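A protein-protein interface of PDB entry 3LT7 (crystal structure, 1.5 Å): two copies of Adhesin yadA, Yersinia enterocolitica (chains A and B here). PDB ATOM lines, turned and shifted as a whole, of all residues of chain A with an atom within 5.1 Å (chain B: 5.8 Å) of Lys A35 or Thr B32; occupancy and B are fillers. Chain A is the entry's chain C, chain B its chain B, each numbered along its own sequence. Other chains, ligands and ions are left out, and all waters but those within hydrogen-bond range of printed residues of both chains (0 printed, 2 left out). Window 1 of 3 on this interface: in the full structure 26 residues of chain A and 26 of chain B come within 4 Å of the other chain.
OD1 of Asp B33 is in hydrogen-bond range of OH of Tyr A31 (2.7 Å).
OG1 of Thr B32 lies within hydrogen-bond range of OG1 of Thr A32, at 3.3 Å.
OD1 of Asp B33 is in salt-bridge range of NZ of Lys A35.
Ser A28 touches Ser B28 (OG to CB, 3.6 Å).
OD1 of Asn B29 touches CA of Ser A28, at 3.5 Å.
Tyr A31 touches Asn B29.
Lys A35 touches Thr B32 (CG to CG2, 3.8 Å).
Lys A35 touches Phe B36 (O to CE2, 3.5 Å).
Phe B36 touches Gln A38.
Leu A39 touches Phe B36 (CD1 to CD2, 3.4 Å).
The side-chain hydroxyl (OG1) of Thr A32 lies within hydrogen-bond range of the backbone carbonyl oxygen (O) of Ser A28 (3.1 Å).
The side-chain amino group (NZ) of Lys A35 is in hydrogen-bond range of the side-chain hydroxyl (OH) of Tyr A31 (2.5 Å).
The backbone carbonyl oxygen (O) of Ser B28 lies within hydrogen-bond range of the side-chain hydroxyl (OG1) of Thr B32, 3.3 Å away.
A ring nitrogen (NE2) of His A34 sits close to the side-chain amide nitrogen (NE2) of Gln A38 (3.4 Å).
Ser B28 touches its own counterpart, Ser A28.
Tyr A31 touches Asp B33, but with the chains exchanged Asp A33 does not touch Tyr B31 (10.8 Å).
Lys A35 touches Thr B32, but with the chains exchanged Thr A32 does not touch Lys B35 (8.5 Å).
Lys A35 touches Phe B36, but with the chains exchanged Phe A36 does not touch Lys B35 (9.0 Å).
8 positions are printed for both chains.
Of the 10 pairs that touch across the chains among the printed residues, 2 have their exchanged pair printed and touching as well.
Of the 11 printed residues of chain B, 5 touch a printed residue of chain A.
Among the printed residues, 10 pairs touch across the chains.
Thr B32 touches just these residues of chain A: Thr A32 and Lys A35.
Of the printed residues of chain A, Asp B33 touches Tyr A31 and Lys A35.
Printed residues of chain A within 4 Å of Asn B29: Ser A28 (3.5 Å) and Tyr A31 (3.4 Å).
Printed residues of chain B within 4 Å of Leu A39: Phe B36.
Of the printed residues of chain A, Phe B36 touches Lys A35 (3.5 Å), Gln A38 (3.7 Å) and Leu A39 (3.4 Å).
Of the printed residues of chain B, Gln A38 touches Phe B36 (3.7 Å).
His B34 touches none of the printed residues of chain A.
Gln B30 touches none of the printed residues of chain A.
The nearest residue of chain B that does not touch Lys A35 is His B37 (5.7 Å).
The nearest printed residue of chain B that does not touch Thr A32 is Asn B29 (5.3 Å).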
ATOM      1  N   SER A  28       8.163   1.170  -4.471  1.00  0.00           N
ATOM      2  CA  SER A  28       8.753   0.468  -5.598  1.00  0.00           C
ATOM      3  C   SER A  28       7.983  -0.732  -6.153  1.00  0.00           C
ATOM      4  O   SER A  28       7.749  -0.913  -7.373  1.00  0.00           O
ATOM      5  CB  SER A  28      10.135   0.050  -5.139  1.00  0.00           C
ATOM      6  OG  SER A  28      10.901   1.245  -5.065  1.00  0.00           O
ATOM      7  N   TYR A  31       4.996   0.211  -7.886  1.00  0.00           N
ATOM      8  CA  TYR A  31       5.257   0.599  -9.286  1.00  0.00           C
ATOM      9  C   TYR A  31       5.467  -0.648 -10.173  1.00  0.00           C
ATOM     10  O   TYR A  31       4.868  -0.782 -11.248  1.00  0.00           O
ATOM     11  CB  TYR A  31       6.430   1.571  -9.324  1.00  0.00           C
ATOM     12  CG  TYR A  31       6.863   1.941 -10.727  1.00  0.00           C
ATOM     13  CD1 TYR A  31       6.220   2.948 -11.429  1.00  0.00           C
ATOM     14  CD2 TYR A  31       7.915   1.289 -11.318  1.00  0.00           C
ATOM     15  CE1 TYR A  31       6.609   3.280 -12.722  1.00  0.00           C
ATOM     16  CE2 TYR A  31       8.332   1.620 -12.632  1.00  0.00           C
ATOM     17  CZ  TYR A  31       7.692   2.620 -13.295  1.00  0.00           C
ATOM     18  OH  TYR A  31       8.135   2.947 -14.535  1.00  0.00           O
ATOM     19  N   THR A  32       6.355  -1.542  -9.760  1.00  0.00           N
ATOM     20  CA  THR A  32       6.355  -2.897 -10.305  1.00  0.00           C
ATOM     21  C   THR A  32       4.950  -3.444 -10.668  1.00  0.00           C
ATOM     22  O   THR A  32       4.766  -3.928 -11.795  1.00  0.00           O
ATOM     23  CB  THR A  32       6.966  -3.856  -9.310  1.00  0.00           C
ATOM     24  OG1 THR A  32       8.309  -3.445  -9.099  1.00  0.00           O
ATOM     25  CG2 THR A  32       6.902  -5.296  -9.782  1.00  0.00           C
ATOM     26  N   ASP A  33       3.952  -3.310  -9.744  1.00  0.00           N
ATOM     27  CA  ASP A  33       2.644  -3.952  -9.879  1.00  0.00           C
ATOM     28  C   ASP A  33       1.926  -3.304 -11.017  1.00  0.00           C
ATOM     29  O   ASP A  33       1.159  -3.962 -11.751  1.00  0.00           O
ATOM     30  CB  ASP A  33       1.816  -3.783  -8.609  1.00  0.00           C
ATOM     31  CG  ASP A  33       2.239  -4.710  -7.540  1.00  0.00           C
ATOM     32  OD1 ASP A  33       2.976  -5.653  -7.884  1.00  0.00           O
ATOM     33  OD2 ASP A  33       1.807  -4.528  -6.371  1.00  0.00           O
ATOM     34  N   HIS A  34       2.196  -2.006 -11.171  1.00  0.00           N
ATOM     35  CA  HIS A  34       1.515  -1.245 -12.185  1.00  0.00           C
ATOM     36  C   HIS A  34       2.094  -1.650 -13.552  1.00  0.00           C
ATOM     37  O   HIS A  34       1.372  -1.717 -14.537  1.00  0.00           O
ATOM     38  CB  HIS A  34       1.638   0.251 -11.900  1.00  0.00           C
ATOM     39  CG  HIS A  34       1.728   1.091 -13.143  1.00  0.00           C
ATOM     40  ND1 HIS A  34       0.713   1.156 -14.072  1.00  0.00           N
ATOM     41  CD2 HIS A  34       2.720   1.883 -13.612  1.00  0.00           C
ATOM     42  CE1 HIS A  34       1.068   1.975 -15.048  1.00  0.00           C
ATOM     43  NE2 HIS A  34       2.280   2.429 -14.793  1.00  0.00           N
ATOM     44  N   LYS A  35       3.403  -1.951 -13.570  1.00  0.00           N
ATOM     45  CA  LYS A  35       4.067  -2.336 -14.768  1.00  0.00           C
ATOM     46  C   LYS A  35       3.714  -3.780 -15.114  1.00  0.00           C
ATOM     47  O   LYS A  35       3.521  -4.079 -16.249  1.00  0.00           O
ATOM     48  CB  LYS A  35       5.575  -2.196 -14.642  1.00  0.00           C
ATOM     49  CG  LYS A  35       6.098  -0.852 -14.166  1.00  0.00           C
ATOM     50  CD  LYS A  35       5.828   0.271 -15.187  1.00  0.00           C
ATOM     51  CE  LYS A  35       6.888   0.322 -16.264  1.00  0.00           C
ATOM     52  NZ  LYS A  35       7.391   1.688 -16.552  1.00  0.00           N
ATOM     53  N   PHE A  36       3.634  -4.683 -14.131  1.00  0.00           N
ATOM     54  CA  PHE A  36       3.163  -6.054 -14.310  1.00  0.00           C
ATOM     55  C   PHE A  36       1.769  -6.083 -14.941  1.00  0.00           C
ATOM     56  O   PHE A  36       1.522  -6.860 -15.853  1.00  0.00           O
ATOM     57  CB  PHE A  36       3.186  -6.743 -12.951  1.00  0.00           C
ATOM     58  CG  PHE A  36       2.621  -8.119 -12.882  1.00  0.00           C
ATOM     59  CD1 PHE A  36       3.464  -9.246 -13.049  1.00  0.00           C
ATOM     60  CD2 PHE A  36       1.278  -8.330 -12.583  1.00  0.00           C
ATOM     61  CE1 PHE A  36       2.964 -10.539 -12.939  1.00  0.00           C
ATOM     62  CE2 PHE A  36       0.771  -9.637 -12.482  1.00  0.00           C
ATOM     63  CZ  PHE A  36       1.604 -10.732 -12.620  1.00  0.00           C
ATOM     64  N   HIS A  37       0.857  -5.223 -14.441  1.00  0.00           N
ATOM     65  CA  HIS A  37      -0.496  -5.179 -15.007  1.00  0.00           C
ATOM     66  C   HIS A  37      -0.539  -4.776 -16.494  1.00  0.00           C
ATOM     67  O   HIS A  37      -1.441  -5.230 -17.241  1.00  0.00           O
ATOM     68  CB  HIS A  37      -1.448  -4.234 -14.231  1.00  0.00           C
ATOM     69  CG  HIS A  37      -1.683  -4.583 -12.795  1.00  0.00           C
ATOM     70  ND1 HIS A  37      -2.200  -3.646 -11.912  1.00  0.00           N
ATOM     71  CD2 HIS A  37      -1.557  -5.724 -12.104  1.00  0.00           C
ATOM     72  CE1 HIS A  37      -2.334  -4.206 -10.720  1.00  0.00           C
ATOM     73  NE2 HIS A  37      -1.916  -5.455 -10.807  1.00  0.00           N
ATOM     74  N   GLN A  38       0.359  -3.871 -16.857  1.00  0.00           N
ATOM     75  CA  GLN A  38       0.368  -3.307 -18.218  1.00  0.00           C
ATOM     76  C   GLN A  38       0.829  -4.428 -19.179  1.00  0.00           C
ATOM     77  O   GLN A  38       0.182  -4.705 -20.209  1.00  0.00           O
ATOM     78  CB  GLN A  38       1.319  -2.123 -18.270  1.00  0.00           C
ATOM     79  CG  GLN A  38       0.800  -0.869 -17.660  1.00  0.00           C
ATOM     80  CD  GLN A  38       1.801   0.281 -17.725  1.00  0.00           C
ATOM     81  OE1 GLN A  38       3.021   0.087 -17.579  1.00  0.00           O
ATOM     82  NE2 GLN A  38       1.287   1.492 -17.923  1.00  0.00           N
ATOM     83  N   LEU A  39       1.922  -5.093 -18.822  1.00  0.00           N
ATOM     84  CA  LEU A  39       2.315  -6.342 -19.511  1.00  0.00           C
ATOM     85  C   LEU A  39       1.214  -7.410 -19.582  1.00  0.00           C
ATOM     86  O   LEU A  39       1.033  -8.026 -20.635  1.00  0.00           O
ATOM     87  CB  LEU A  39       3.584  -6.946 -18.891  1.00  0.00           C
ATOM     88  CG  LEU A  39       4.775  -6.025 -19.033  1.00  0.00           C
ATOM     89  CD1 LEU A  39       5.966  -6.444 -18.119  1.00  0.00           C
ATOM     90  CD2 LEU A  39       5.150  -5.829 -20.535  1.00  0.00           C
ATOM     91  N   GLU B  27      16.166   4.199  -8.131  1.00  0.00           N
ATOM     92  CA  GLU B  27      16.954   3.062  -8.566  1.00  0.00           C
ATOM     93  C   GLU B  27      16.126   1.776  -8.759  1.00  0.00           C
ATOM     94  O   GLU B  27      16.352   1.006  -9.718  1.00  0.00           O
ATOM     95  CB  GLU B  27      18.173   2.871  -7.654  1.00  0.00           C
ATOM     96  CG  GLU B  27      19.396   3.766  -8.088  1.00  0.00           C
ATOM     97  CD  GLU B  27      20.728   3.480  -7.352  1.00  0.00           C
ATOM     98  OE1 GLU B  27      21.044   2.310  -7.076  1.00  0.00           O
ATOM     99  OE2 GLU B  27      21.480   4.431  -7.061  1.00  0.00           O
ATOM    100  N   SER B  28      15.220   1.493  -7.835  1.00  0.00           N
ATOM    101  CA  SER B  28      14.483   0.241  -7.981  1.00  0.00           C
ATOM    102  C   SER B  28      13.574   0.325  -9.211  1.00  0.00           C
ATOM    103  O   SER B  28      13.471  -0.649 -10.007  1.00  0.00           O
ATOM    104  CB  SER B  28      13.718  -0.173  -6.737  1.00  0.00           C
ATOM    105  OG  SER B  28      14.513  -0.303  -5.594  1.00  0.00           O
ATOM    106  N   ASN B  29      12.943   1.500  -9.396  1.00  0.00           N
ATOM    107  CA  ASN B  29      12.056   1.689 -10.534  1.00  0.00           C
ATOM    108  C   ASN B  29      12.815   1.612 -11.861  1.00  0.00           C
ATOM    109  O   ASN B  29      12.269   1.019 -12.802  1.00  0.00           O
ATOM    110  CB  ASN B  29      11.206   2.961 -10.377  1.00  0.00           C
ATOM    111  CG  ASN B  29      10.191   2.835  -9.278  1.00  0.00           C
ATOM    112  OD1 ASN B  29      10.195   1.848  -8.517  1.00  0.00           O
ATOM    113  ND2 ASN B  29       9.320   3.837  -9.160  1.00  0.00           N
ATOM    114  N   GLN B  30      14.096   2.071 -11.886  1.00  0.00           N
ATOM    115  CA  GLN B  30      14.936   1.917 -13.086  1.00  0.00           C
ATOM    116  C   GLN B  30      15.121   0.430 -13.440  1.00  0.00           C
ATOM    117  O   GLN B  30      15.114   0.024 -14.604  1.00  0.00           O
ATOM    118  CB  GLN B  30      16.315   2.553 -12.900  1.00  0.00           C
ATOM    119  CG  GLN B  30      16.297   4.053 -13.170  1.00  0.00           C
ATOM    120  CD  GLN B  30      17.567   4.783 -12.718  1.00  0.00           C
ATOM    121  OE1 GLN B  30      18.299   5.333 -13.536  1.00  0.00           O
ATOM    122  NE2 GLN B  30      17.786   4.856 -11.400  1.00  0.00           N
ATOM    123  N   TYR B  31      15.273  -0.367 -12.396  1.00  0.00           N
ATOM    124  CA  TYR B  31      15.422  -1.783 -12.517  1.00  0.00           C
ATOM    125  C   TYR B  31      14.181  -2.354 -13.172  1.00  0.00           C
ATOM    126  O   TYR B  31      14.285  -3.052 -14.187  1.00  0.00           O
ATOM    127  CB  TYR B  31      15.625  -2.451 -11.156  1.00  0.00           C
ATOM    128  CG  TYR B  31      16.000  -3.924 -11.283  1.00  0.00           C
ATOM    129  CD1 TYR B  31      17.321  -4.353 -11.565  1.00  0.00           C
ATOM    130  CD2 TYR B  31      15.024  -4.886 -11.098  1.00  0.00           C
ATOM    131  CE1 TYR B  31      17.627  -5.717 -11.683  1.00  0.00           C
ATOM    132  CE2 TYR B  31      15.311  -6.214 -11.181  1.00  0.00           C
ATOM    133  CZ  TYR B  31      16.608  -6.646 -11.470  1.00  0.00           C
ATOM    134  OH  TYR B  31      16.753  -8.000 -11.555  1.00  0.00           O
ATOM    135  N   THR B  32      13.024  -2.049 -12.584  1.00  0.00           N
ATOM    136  CA  THR B  32      11.753  -2.488 -13.147  1.00  0.00           C
ATOM    137  C   THR B  32      11.545  -2.055 -14.601  1.00  0.00           C
ATOM    138  O   THR B  32      11.000  -2.809 -15.402  1.00  0.00           O
ATOM    139  CB  THR B  32      10.595  -1.946 -12.321  1.00  0.00           C
ATOM    140  OG1 THR B  32      10.767  -2.366 -10.959  1.00  0.00           O
ATOM    141  CG2 THR B  32       9.258  -2.452 -12.851  1.00  0.00           C
ATOM    142  N   ASP B  33      11.904  -0.799 -14.892  1.00  0.00           N
ATOM    143  CA  ASP B  33      11.779  -0.199 -16.246  1.00  0.00           C
ATOM    144  C   ASP B  33      12.557  -0.992 -17.280  1.00  0.00           C
ATOM    145  O   ASP B  33      12.107  -1.174 -18.406  1.00  0.00           O
ATOM    146  CB  ASP B  33      12.346   1.198 -16.267  1.00  0.00           C
ATOM    147  CG  ASP B  33      11.303   2.237 -16.017  1.00  0.00           C
ATOM    148  OD1 ASP B  33      10.096   1.885 -16.043  1.00  0.00           O
ATOM    149  OD2 ASP B  33      11.673   3.411 -15.765  1.00  0.00           O
ATOM    150  N   HIS B  34      13.749  -1.395 -16.905  1.00  0.00           N
ATOM    151  CA  HIS B  34      14.633  -2.088 -17.808  1.00  0.00           C
ATOM    152  C   HIS B  34      14.050  -3.457 -18.081  1.00  0.00           C
ATOM    153  O   HIS B  34      13.923  -3.825 -19.229  1.00  0.00           O
ATOM    154  CB  HIS B  34      16.062  -2.166 -17.270  1.00  0.00           C
ATOM    155  CG  HIS B  34      16.768  -0.844 -17.198  1.00  0.00           C
ATOM    156  ND1 HIS B  34      18.125  -0.746 -16.966  1.00  0.00           N
ATOM    157  CD2 HIS B  34      16.327   0.432 -17.349  1.00  0.00           C
ATOM    158  CE1 HIS B  34      18.486   0.525 -16.949  1.00  0.00           C
ATOM    159  NE2 HIS B  34      17.414   1.262 -17.184  1.00  0.00           N
ATOM    160  N   LYS B  35      13.644  -4.180 -17.032  1.00  0.00           N
ATOM    161  CA  LYS B  35      13.028  -5.498 -17.197  1.00  0.00           C
ATOM    162  C   LYS B  35      11.708  -5.451 -18.001  1.00  0.00           C
ATOM    163  O   LYS B  35      11.382  -6.369 -18.733  1.00  0.00           O
ATOM    164  CB  LYS B  35      12.873  -6.203 -15.832  1.00  0.00           C
ATOM    165  CG  LYS B  35      14.215  -6.404 -15.054  1.00  0.00           C
ATOM    166  CD  LYS B  35      15.088  -7.636 -15.486  1.00  0.00           C
ATOM    167  CE  LYS B  35      15.118  -8.740 -14.376  1.00  0.00           C
ATOM    168  NZ  LYS B  35      16.420  -9.523 -14.324  1.00  0.00           N
ATOM    169  N   PHE B  36      10.961  -4.365 -17.832  1.00  0.00           N
ATOM    170  CA  PHE B  36       9.695  -4.136 -18.527  1.00  0.00           C
ATOM    171  C   PHE B  36       9.906  -3.922 -20.009  1.00  0.00           C
ATOM    172  O   PHE B  36       9.208  -4.519 -20.824  1.00  0.00           O
ATOM    173  CB  PHE B  36       9.078  -2.886 -17.934  1.00  0.00           C
ATOM    174  CG  PHE B  36       7.809  -2.459 -18.588  1.00  0.00           C
ATOM    175  CD1 PHE B  36       7.804  -1.394 -19.482  1.00  0.00           C
ATOM    176  CD2 PHE B  36       6.599  -3.088 -18.283  1.00  0.00           C
ATOM    177  CE1 PHE B  36       6.607  -0.966 -20.057  1.00  0.00           C
ATOM    178  CE2 PHE B  36       5.409  -2.667 -18.865  1.00  0.00           C
ATOM    179  CZ  PHE B  36       5.421  -1.610 -19.761  1.00  0.00           C
ATOM    180  N   HIS B  37      10.846  -3.044 -20.353  1.00  0.00           N
ATOM    181  CA  HIS B  37      11.292  -2.868 -21.752  1.00  0.00           C
ATOM    182  C   HIS B  37      11.697  -4.179 -22.434  1.00  0.00           C
ATOM    183  O   HIS B  37      11.201  -4.479 -23.537  1.00  0.00           O
ATOM    184  CB  HIS B  37      12.461  -1.900 -21.811  1.00  0.00           C
ATOM    185  CG  HIS B  37      12.048  -0.492 -21.565  1.00  0.00           C
ATOM    186  ND1 HIS B  37      12.644   0.589 -22.176  1.00  0.00           N
ATOM    187  CD2 HIS B  37      11.077   0.010 -20.766  1.00  0.00           C
ATOM    188  CE1 HIS B  37      12.055   1.698 -21.765  1.00  0.00           C
ATOM    189  NE2 HIS B  37      11.102   1.374 -20.908  1.00  0.00           N
